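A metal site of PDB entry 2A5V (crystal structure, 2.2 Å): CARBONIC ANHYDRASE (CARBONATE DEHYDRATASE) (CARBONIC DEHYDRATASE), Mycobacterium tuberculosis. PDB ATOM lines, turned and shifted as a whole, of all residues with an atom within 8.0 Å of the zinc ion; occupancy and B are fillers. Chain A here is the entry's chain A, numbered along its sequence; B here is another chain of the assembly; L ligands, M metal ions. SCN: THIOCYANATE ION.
Three residues have an atom within 4 Å of the zinc ion: Cys 57, His 110 and Cys 113.
The nearest printed residue that does not touch the zinc ion is Asp 59 (4.04 Å).
The zinc ion is bound by a nitrogen (N) of the ligand (1.9 Å).
NE2 of His 110 is bound to the zinc ion.
The side-chain sulfur (SG) of Cys 113 is bound to the zinc ion, at 2.3 Å.
The side-chain sulfur (SG) of Cys 57 is bound to the zinc ion, 2.4 Å away.
SG of Cys 113 lies close to N of Ala 115 (3.7 Å).
The side-chain sulfur (SG) of Cys 113 lies close to the backbone NH (N) of Val 116, 3.8 Å away.
The backbone NH (N) of Cys 113 is in hydrogen-bond range of the side-chain carboxylate (OE2) of Glu 159, 3.2 Å away.
The backbone carbonyl oxygen of Cys 113 lies within hydrogen-bond range of the side-chain amide nitrogen of Asn 117, 3.3 Å away.
SG of Cys 57 lies close to N of Asp 59.
The side-chain sulfur (SG) of Cys 57 sits close to the backbone NH (N) of Gly 82, at 3.3 Å.
N of Cys 57 lies within hydrogen-bond range of O of Leu 108 (3.5 Å).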
ATOM      1  N   GLY A  56      26.049  12.201  -1.850  1.00  0.00           N
ATOM      2  CA  GLY A  56      25.468  11.598  -0.672  1.00  0.00           C
ATOM      3  C   GLY A  56      26.396  10.588  -0.065  1.00  0.00           C
ATOM      4  O   GLY A  56      27.455  10.312  -0.607  1.00  0.00           O
ATOM      5  N   CYS A  57      26.018  10.074   1.091  1.00  0.00           N
ATOM      6  CA  CYS A  57      26.693   8.942   1.662  1.00  0.00           C
ATOM      7  C   CYS A  57      26.348   7.623   0.937  1.00  0.00           C
ATOM      8  O   CYS A  57      25.229   7.457   0.440  1.00  0.00           O
ATOM      9  CB  CYS A  57      26.357   8.815   3.149  1.00  0.00           C
ATOM     10  SG  CYS A  57      27.340   7.508   3.942  1.00  0.00           S
ATOM     11  N   ALA A  58      27.300   6.693   0.916  1.00  0.00           N
ATOM     12  CA  ALA A  58      27.122   5.346   0.358  1.00  0.00           C
ATOM     13  C   ALA A  58      26.187   4.443   1.179  1.00  0.00           C
ATOM     14  O   ALA A  58      25.757   3.388   0.712  1.00  0.00           O
ATOM     15  CB  ALA A  58      28.491   4.689   0.165  1.00  0.00           C
ATOM     16  N   ASP A  59      25.832   4.876   2.380  1.00  0.00           N
ATOM     17  CA  ASP A  59      24.965   4.119   3.252  1.00  0.00           C
ATOM     18  C   ASP A  59      23.753   3.575   2.462  1.00  0.00           C
ATOM     19  O   ASP A  59      23.086   4.318   1.743  1.00  0.00           O
ATOM     20  CB  ASP A  59      24.541   5.006   4.434  1.00  0.00           C
ATOM     21  CG  ASP A  59      23.786   4.241   5.530  1.00  0.00           C
ATOM     22  OD1 ASP A  59      22.701   3.692   5.276  1.00  0.00           O
ATOM     23  OD2 ASP A  59      24.292   4.194   6.661  1.00  0.00           O
ATOM     24  N   SER A  60      23.501   2.263   2.592  1.00  0.00           N
ATOM     25  CA  SER A  60      22.456   1.586   1.847  1.00  0.00           C
ATOM     26  C   SER A  60      21.049   2.029   2.197  1.00  0.00           C
ATOM     27  O   SER A  60      20.086   1.678   1.498  1.00  0.00           O
ATOM     28  CB  SER A  60      22.578   0.076   2.052  1.00  0.00           C
ATOM     29  OG  SER A  60      22.260  -0.274   3.377  1.00  0.00           O
ATOM     30  N   ARG A  61      20.900   2.806   3.264  1.00  0.00           N
ATOM     31  CA  ARG A  61      19.580   3.282   3.684  1.00  0.00           C
ATOM     32  C   ARG A  61      19.287   4.674   3.122  1.00  0.00           C
ATOM     33  O   ARG A  61      18.173   5.179   3.253  1.00  0.00           O
ATOM     34  CB  ARG A  61      19.449   3.262   5.207  1.00  0.00           C
ATOM     35  CG  ARG A  61      19.645   1.882   5.866  1.00  0.00           C
ATOM     36  CD  ARG A  61      19.923   2.052   7.354  1.00  0.00           C
ATOM     37  NE  ARG A  61      21.232   2.671   7.629  1.00  0.00           N
ATOM     38  CZ  ARG A  61      21.705   2.913   8.846  1.00  0.00           C
ATOM     39  NH1 ARG A  61      20.987   2.616   9.935  1.00  0.00           N
ATOM     40  NH2 ARG A  61      22.896   3.451   8.973  1.00  0.00           N
ATOM     41  N   VAL A  62      20.286   5.285   2.486  1.00  0.00           N
ATOM     42  CA  VAL A  62      20.141   6.639   1.981  1.00  0.00           C
ATOM     43  C   VAL A  62      20.215   6.637   0.448  1.00  0.00           C
ATOM     44  O   VAL A  62      21.020   7.349  -0.171  1.00  0.00           O
ATOM     45  CB  VAL A  62      21.212   7.594   2.604  1.00  0.00           C
ATOM     46  CG1 VAL A  62      20.773   9.038   2.486  1.00  0.00           C
ATOM     47  CG2 VAL A  62      21.400   7.287   4.069  1.00  0.00           C
ATOM     48  N   THR A  80      30.020   8.443  -1.595  1.00  0.00           N
ATOM     49  CA  THR A  80      31.156   7.824  -0.864  1.00  0.00           C
ATOM     50  C   THR A  80      30.767   7.690   0.602  1.00  0.00           C
ATOM     51  O   THR A  80      29.789   8.313   1.059  1.00  0.00           O
ATOM     52  CB  THR A  80      32.495   8.643  -0.956  1.00  0.00           C
ATOM     53  OG1 THR A  80      32.272   9.986  -0.508  1.00  0.00           O
ATOM     54  CG2 THR A  80      33.045   8.676  -2.390  1.00  0.00           C
ATOM     55  N   ALA A  81      31.505   6.862   1.351  1.00  0.00           N
ATOM     56  CA  ALA A  81      31.252   6.708   2.782  1.00  0.00           C
ATOM     57  C   ALA A  81      31.480   8.052   3.492  1.00  0.00           C
ATOM     58  O   ALA A  81      32.539   8.654   3.370  1.00  0.00           O
ATOM     59  CB  ALA A  81      32.127   5.608   3.365  1.00  0.00           C
ATOM     60  N   GLY A  82      30.449   8.531   4.189  1.00  0.00           N
ATOM     61  CA  GLY A  82      30.497   9.787   4.912  1.00  0.00           C
ATOM     62  C   GLY A  82      30.624  10.988   3.985  1.00  0.00           C
ATOM     63  O   GLY A  82      31.049  12.051   4.452  1.00  0.00           O
ATOM     64  N   HIS A  83      30.234  10.821   2.704  1.00  0.00           N
ATOM     65  CA  HIS A  83      30.404  11.837   1.643  1.00  0.00           C
ATOM     66  C   HIS A  83      31.732  12.601   1.766  1.00  0.00           C
ATOM     67  O   HIS A  83      31.779  13.834   1.768  1.00  0.00           O
ATOM     68  CB  HIS A  83      29.199  12.785   1.516  1.00  0.00           C
ATOM     69  CG  HIS A  83      28.835  13.484   2.794  1.00  0.00           C
ATOM     70  ND1 HIS A  83      29.574  14.520   3.312  1.00  0.00           N
ATOM     71  CD2 HIS A  83      27.832  13.261   3.670  1.00  0.00           C
ATOM     72  CE1 HIS A  83      29.029  14.922   4.450  1.00  0.00           C
ATOM     73  NE2 HIS A  83      27.970  14.181   4.683  1.00  0.00           N
ATOM     74  N   LEU A 108      24.430  15.455   0.907  1.00  0.00           N
ATOM     75  CA  LEU A 108      23.377  14.741   1.630  1.00  0.00           C
ATOM     76  C   LEU A 108      23.980  13.922   2.775  1.00  0.00           C
ATOM     77  O   LEU A 108      24.551  12.886   2.543  1.00  0.00           O
ATOM     78  CB  LEU A 108      22.574  13.846   0.668  1.00  0.00           C
ATOM     79  CG  LEU A 108      21.383  13.000   1.178  1.00  0.00           C
ATOM     80  CD1 LEU A 108      20.278  13.858   1.823  1.00  0.00           C
ATOM     81  CD2 LEU A 108      20.783  12.147   0.077  1.00  0.00           C
ATOM     82  N   GLY A 109      23.845  14.413   4.007  1.00  0.00           N
ATOM     83  CA  GLY A 109      24.229  13.598   5.156  1.00  0.00           C
ATOM     84  C   GLY A 109      22.995  12.895   5.724  1.00  0.00           C
ATOM     85  O   GLY A 109      21.919  12.999   5.156  1.00  0.00           O
ATOM     86  N   HIS A 110      23.149  12.202   6.837  1.00  0.00           N
ATOM     87  CA  HIS A 110      22.026  11.506   7.437  1.00  0.00           C
ATOM     88  C   HIS A 110      22.423  11.151   8.861  1.00  0.00           C
ATOM     89  O   HIS A 110      23.587  11.189   9.199  1.00  0.00           O
ATOM     90  CB  HIS A 110      21.699  10.215   6.650  1.00  0.00           C
ATOM     91  CG  HIS A 110      22.822   9.224   6.678  1.00  0.00           C
ATOM     92  ND1 HIS A 110      22.806   8.110   7.501  1.00  0.00           N
ATOM     93  CD2 HIS A 110      24.022   9.226   6.066  1.00  0.00           C
ATOM     94  CE1 HIS A 110      23.953   7.462   7.371  1.00  0.00           C
ATOM     95  NE2 HIS A 110      24.695   8.114   6.495  1.00  0.00           N
ATOM     96  N   ASP A 111      21.442  10.761   9.670  1.00  0.00           N
ATOM     97  CA  ASP A 111      21.755  10.328  11.018  1.00  0.00           C
ATOM     98  C   ASP A 111      22.263   8.881  11.067  1.00  0.00           C
ATOM     99  O   ASP A 111      22.002   8.065  10.173  1.00  0.00           O
ATOM    100  CB  ASP A 111      20.568  10.560  11.962  1.00  0.00           C
ATOM    101  CG  ASP A 111      19.396   9.713  11.619  1.00  0.00           C
ATOM    102  OD1 ASP A 111      19.022   9.666  10.419  1.00  0.00           O
ATOM    103  OD2 ASP A 111      18.851   9.060  12.541  1.00  0.00           O
ATOM    104  N   SER A 112      23.010   8.583  12.124  1.00  0.00           N
ATOM    105  CA  SER A 112      23.541   7.245  12.346  1.00  0.00           C
ATOM    106  C   SER A 112      24.535   6.899  11.205  1.00  0.00           C
ATOM    107  O   SER A 112      24.580   5.770  10.675  1.00  0.00           O
ATOM    108  CB  SER A 112      22.340   6.281  12.514  1.00  0.00           C
ATOM    109  OG  SER A 112      22.722   4.918  12.614  1.00  0.00           O
ATOM    110  N   CYS A 113      25.362   7.889  10.845  1.00  0.00           N
ATOM    111  CA  CYS A 113      26.382   7.727   9.801  1.00  0.00           C
ATOM    112  C   CYS A 113      27.615   7.032  10.370  1.00  0.00           C
ATOM    113  O   CYS A 113      28.287   7.562  11.278  1.00  0.00           O
ATOM    114  CB  CYS A 113      26.781   9.086   9.189  1.00  0.00           C
ATOM    115  SG  CYS A 113      28.016   8.980   7.844  1.00  0.00           S
ATOM    116  N   GLY A 114      27.935   5.860   9.821  1.00  0.00           N
ATOM    117  CA  GLY A 114      29.051   5.086  10.363  1.00  0.00           C
ATOM    118  C   GLY A 114      30.419   5.727  10.166  1.00  0.00           C
ATOM    119  O   GLY A 114      31.334   5.424  10.916  1.00  0.00           O
ATOM    120  N   ALA A 115      30.568   6.576   9.148  1.00  0.00           N
ATOM    121  CA  ALA A 115      31.822   7.296   8.891  1.00  0.00           C
ATOM    122  C   ALA A 115      32.018   8.380   9.952  1.00  0.00           C
ATOM    123  O   ALA A 115      33.118   8.539  10.489  1.00  0.00           O
ATOM    124  CB  ALA A 115      31.847   7.901   7.488  1.00  0.00           C
ATOM    125  N   VAL A 116      30.939   9.117  10.256  1.00  0.00           N
ATOM    126  CA  VAL A 116      30.961  10.063  11.375  1.00  0.00           C
ATOM    127  C   VAL A 116      31.166   9.350  12.712  1.00  0.00           C
ATOM    128  O   VAL A 116      31.950   9.821  13.537  1.00  0.00           O
ATOM    129  CB  VAL A 116      29.727  11.006  11.377  1.00  0.00           C
ATOM    130  CG1 VAL A 116      29.686  11.886  12.650  1.00  0.00           C
ATOM    131  CG2 VAL A 116      29.763  11.886  10.143  1.00  0.00           C
ATOM    132  N   ASN A 117      30.537   8.204  12.919  1.00  0.00           N
ATOM    133  CA  ASN A 117      30.763   7.449  14.170  1.00  0.00           C
ATOM    134  C   ASN A 117      32.215   6.965  14.337  1.00  0.00           C
ATOM    135  O   ASN A 117      32.765   7.022  15.450  1.00  0.00           O
ATOM    136  CB  ASN A 117      29.779   6.262  14.341  1.00  0.00           C
ATOM    137  CG  ASN A 117      28.309   6.710  14.508  1.00  0.00           C
ATOM    138  OD1 ASN A 117      28.012   7.739  15.110  1.00  0.00           O
ATOM    139  ND2 ASN A 117      27.386   5.902  13.968  1.00  0.00           N
ATOM    140  N   GLU A 159      27.313  15.311  12.684  1.00  0.00           N
ATOM    141  CA  GLU A 159      26.818  14.920  11.358  1.00  0.00           C
ATOM    142  C   GLU A 159      26.472  16.153  10.527  1.00  0.00           C
ATOM    143  O   GLU A 159      26.749  16.229   9.334  1.00  0.00           O
ATOM    144  CB  GLU A 159      25.586  13.993  11.502  1.00  0.00           C
ATOM    145  CG  GLU A 159      25.978  12.585  12.027  1.00  0.00           C
ATOM    146  CD  GLU A 159      24.814  11.735  12.578  1.00  0.00           C
ATOM    147  OE1 GLU A 159      23.712  12.265  12.898  1.00  0.00           O
ATOM    148  OE2 GLU A 159      25.034  10.498  12.663  1.00  0.00           O
ATOM    149  N   HIS A 162      29.636  18.068   9.690  1.00  0.00           N
ATOM    150  CA  HIS A 162      30.300  17.391   8.578  1.00  0.00           C
ATOM    151  C   HIS A 162      29.753  17.770   7.198  1.00  0.00           C
ATOM    152  O   HIS A 162      30.522  17.961   6.269  1.00  0.00           O
ATOM    153  CB  HIS A 162      30.320  15.859   8.782  1.00  0.00           C
ATOM    154  CG  HIS A 162      31.124  15.118   7.759  1.00  0.00           C
ATOM    155  ND1 HIS A 162      32.423  15.447   7.455  1.00  0.00           N
ATOM    156  CD2 HIS A 162      30.809  14.052   6.974  1.00  0.00           C
ATOM    157  CE1 HIS A 162      32.879  14.635   6.518  1.00  0.00           C
ATOM    158  NE2 HIS A 162      31.922  13.773   6.212  1.00  0.00           N
ATOM    159  N   LEU A 195      16.595   8.902   9.124  1.00  0.00           N
ATOM    160  CA  LEU A 195      16.284   7.496   8.859  1.00  0.00           C
ATOM    161  C   LEU A 195      14.929   7.073   9.460  1.00  0.00           C
ATOM    162  O   LEU A 195      14.292   6.144   8.977  1.00  0.00           O
ATOM    163  CB  LEU A 195      17.393   6.592   9.402  1.00  0.00           C
ATOM    164  CG  LEU A 195      18.877   6.729   9.017  1.00  0.00           C
ATOM    165  CD1 LEU A 195      19.649   5.589   9.661  1.00  0.00           C
ATOM    166  CD2 LEU A 195      19.110   6.752   7.536  1.00  0.00           C
ATOM    167  N   GLN B  48      22.124  -1.265   9.224  1.00  0.00           N
ATOM    168  CA  GLN B  48      22.035  -1.710   7.833  1.00  0.00           C
ATOM    169  C   GLN B  48      22.711  -3.076   7.629  1.00  0.00           C
ATOM    170  O   GLN B  48      23.776  -3.346   8.210  1.00  0.00           O
ATOM    171  CB  GLN B  48      22.636  -0.663   6.870  1.00  0.00           C
ATOM    172  CG  GLN B  48      24.146  -0.471   7.034  1.00  0.00           C
ATOM    173  CD  GLN B  48      24.754   0.521   6.046  1.00  0.00           C
ATOM    174  OE1 GLN B  48      25.519   1.422   6.434  1.00  0.00           O
ATOM    175  NE2 GLN B  48      24.458   0.350   4.768  1.00  0.00           N
ATOM    176  N   PHE B  76      24.910  -1.056  -0.456  1.00  0.00           N
ATOM    177  CA  PHE B  76      25.830   0.056  -0.201  1.00  0.00           C
ATOM    178  C   PHE B  76      26.235   0.575  -1.588  1.00  0.00           C
ATOM    179  O   PHE B  76      26.527  -0.208  -2.481  1.00  0.00           O
ATOM    180  CB  PHE B  76      27.030  -0.512   0.558  1.00  0.00           C
ATOM    181  CG  PHE B  76      27.946   0.517   1.170  1.00  0.00           C
ATOM    182  CD1 PHE B  76      27.632   1.124   2.388  1.00  0.00           C
ATOM    183  CD2 PHE B  76      29.153   0.856   0.552  1.00  0.00           C
ATOM    184  CE1 PHE B  76      28.522   2.034   2.989  1.00  0.00           C
ATOM    185  CE2 PHE B  76      30.054   1.747   1.145  1.00  0.00           C
ATOM    186  CZ  PHE B  76      29.731   2.350   2.362  1.00  0.00           C
ATOM    187  N   TYR B  95      34.976  -0.302   3.283  1.00  0.00           N
ATOM    188  CA  TYR B  95      34.082  -0.197   4.436  1.00  0.00           C
ATOM    189  C   TYR B  95      32.959  -1.248   4.311  1.00  0.00           C
ATOM    190  O   TYR B  95      32.661  -1.956   5.264  1.00  0.00           O
ATOM    191  CB  TYR B  95      33.513   1.222   4.567  1.00  0.00           C
ATOM    192  CG  TYR B  95      32.626   1.357   5.758  1.00  0.00           C
ATOM    193  CD1 TYR B  95      33.119   1.850   6.955  1.00  0.00           C
ATOM    194  CD2 TYR B  95      31.288   0.962   5.706  1.00  0.00           C
ATOM    195  CE1 TYR B  95      32.302   1.938   8.082  1.00  0.00           C
ATOM    196  CE2 TYR B  95      30.458   1.053   6.821  1.00  0.00           C
ATOM    197  CZ  TYR B  95      30.965   1.540   7.999  1.00  0.00           C
ATOM    198  OH  TYR B  95      30.136   1.629   9.085  1.00  0.00           O
HETATM  199  S   SCN L   1      29.413   4.570   5.948  1.00  0.00           S
HETATM  200  C   SCN L   1      27.897   5.436   6.311  1.00  0.00           C
HETATM  201  N   SCN L   1      26.917   6.017   6.681  1.00  0.00           N
HETATM  202 ZN    ZN M   1      26.791   7.834   6.240  1.00  0.00          ZN
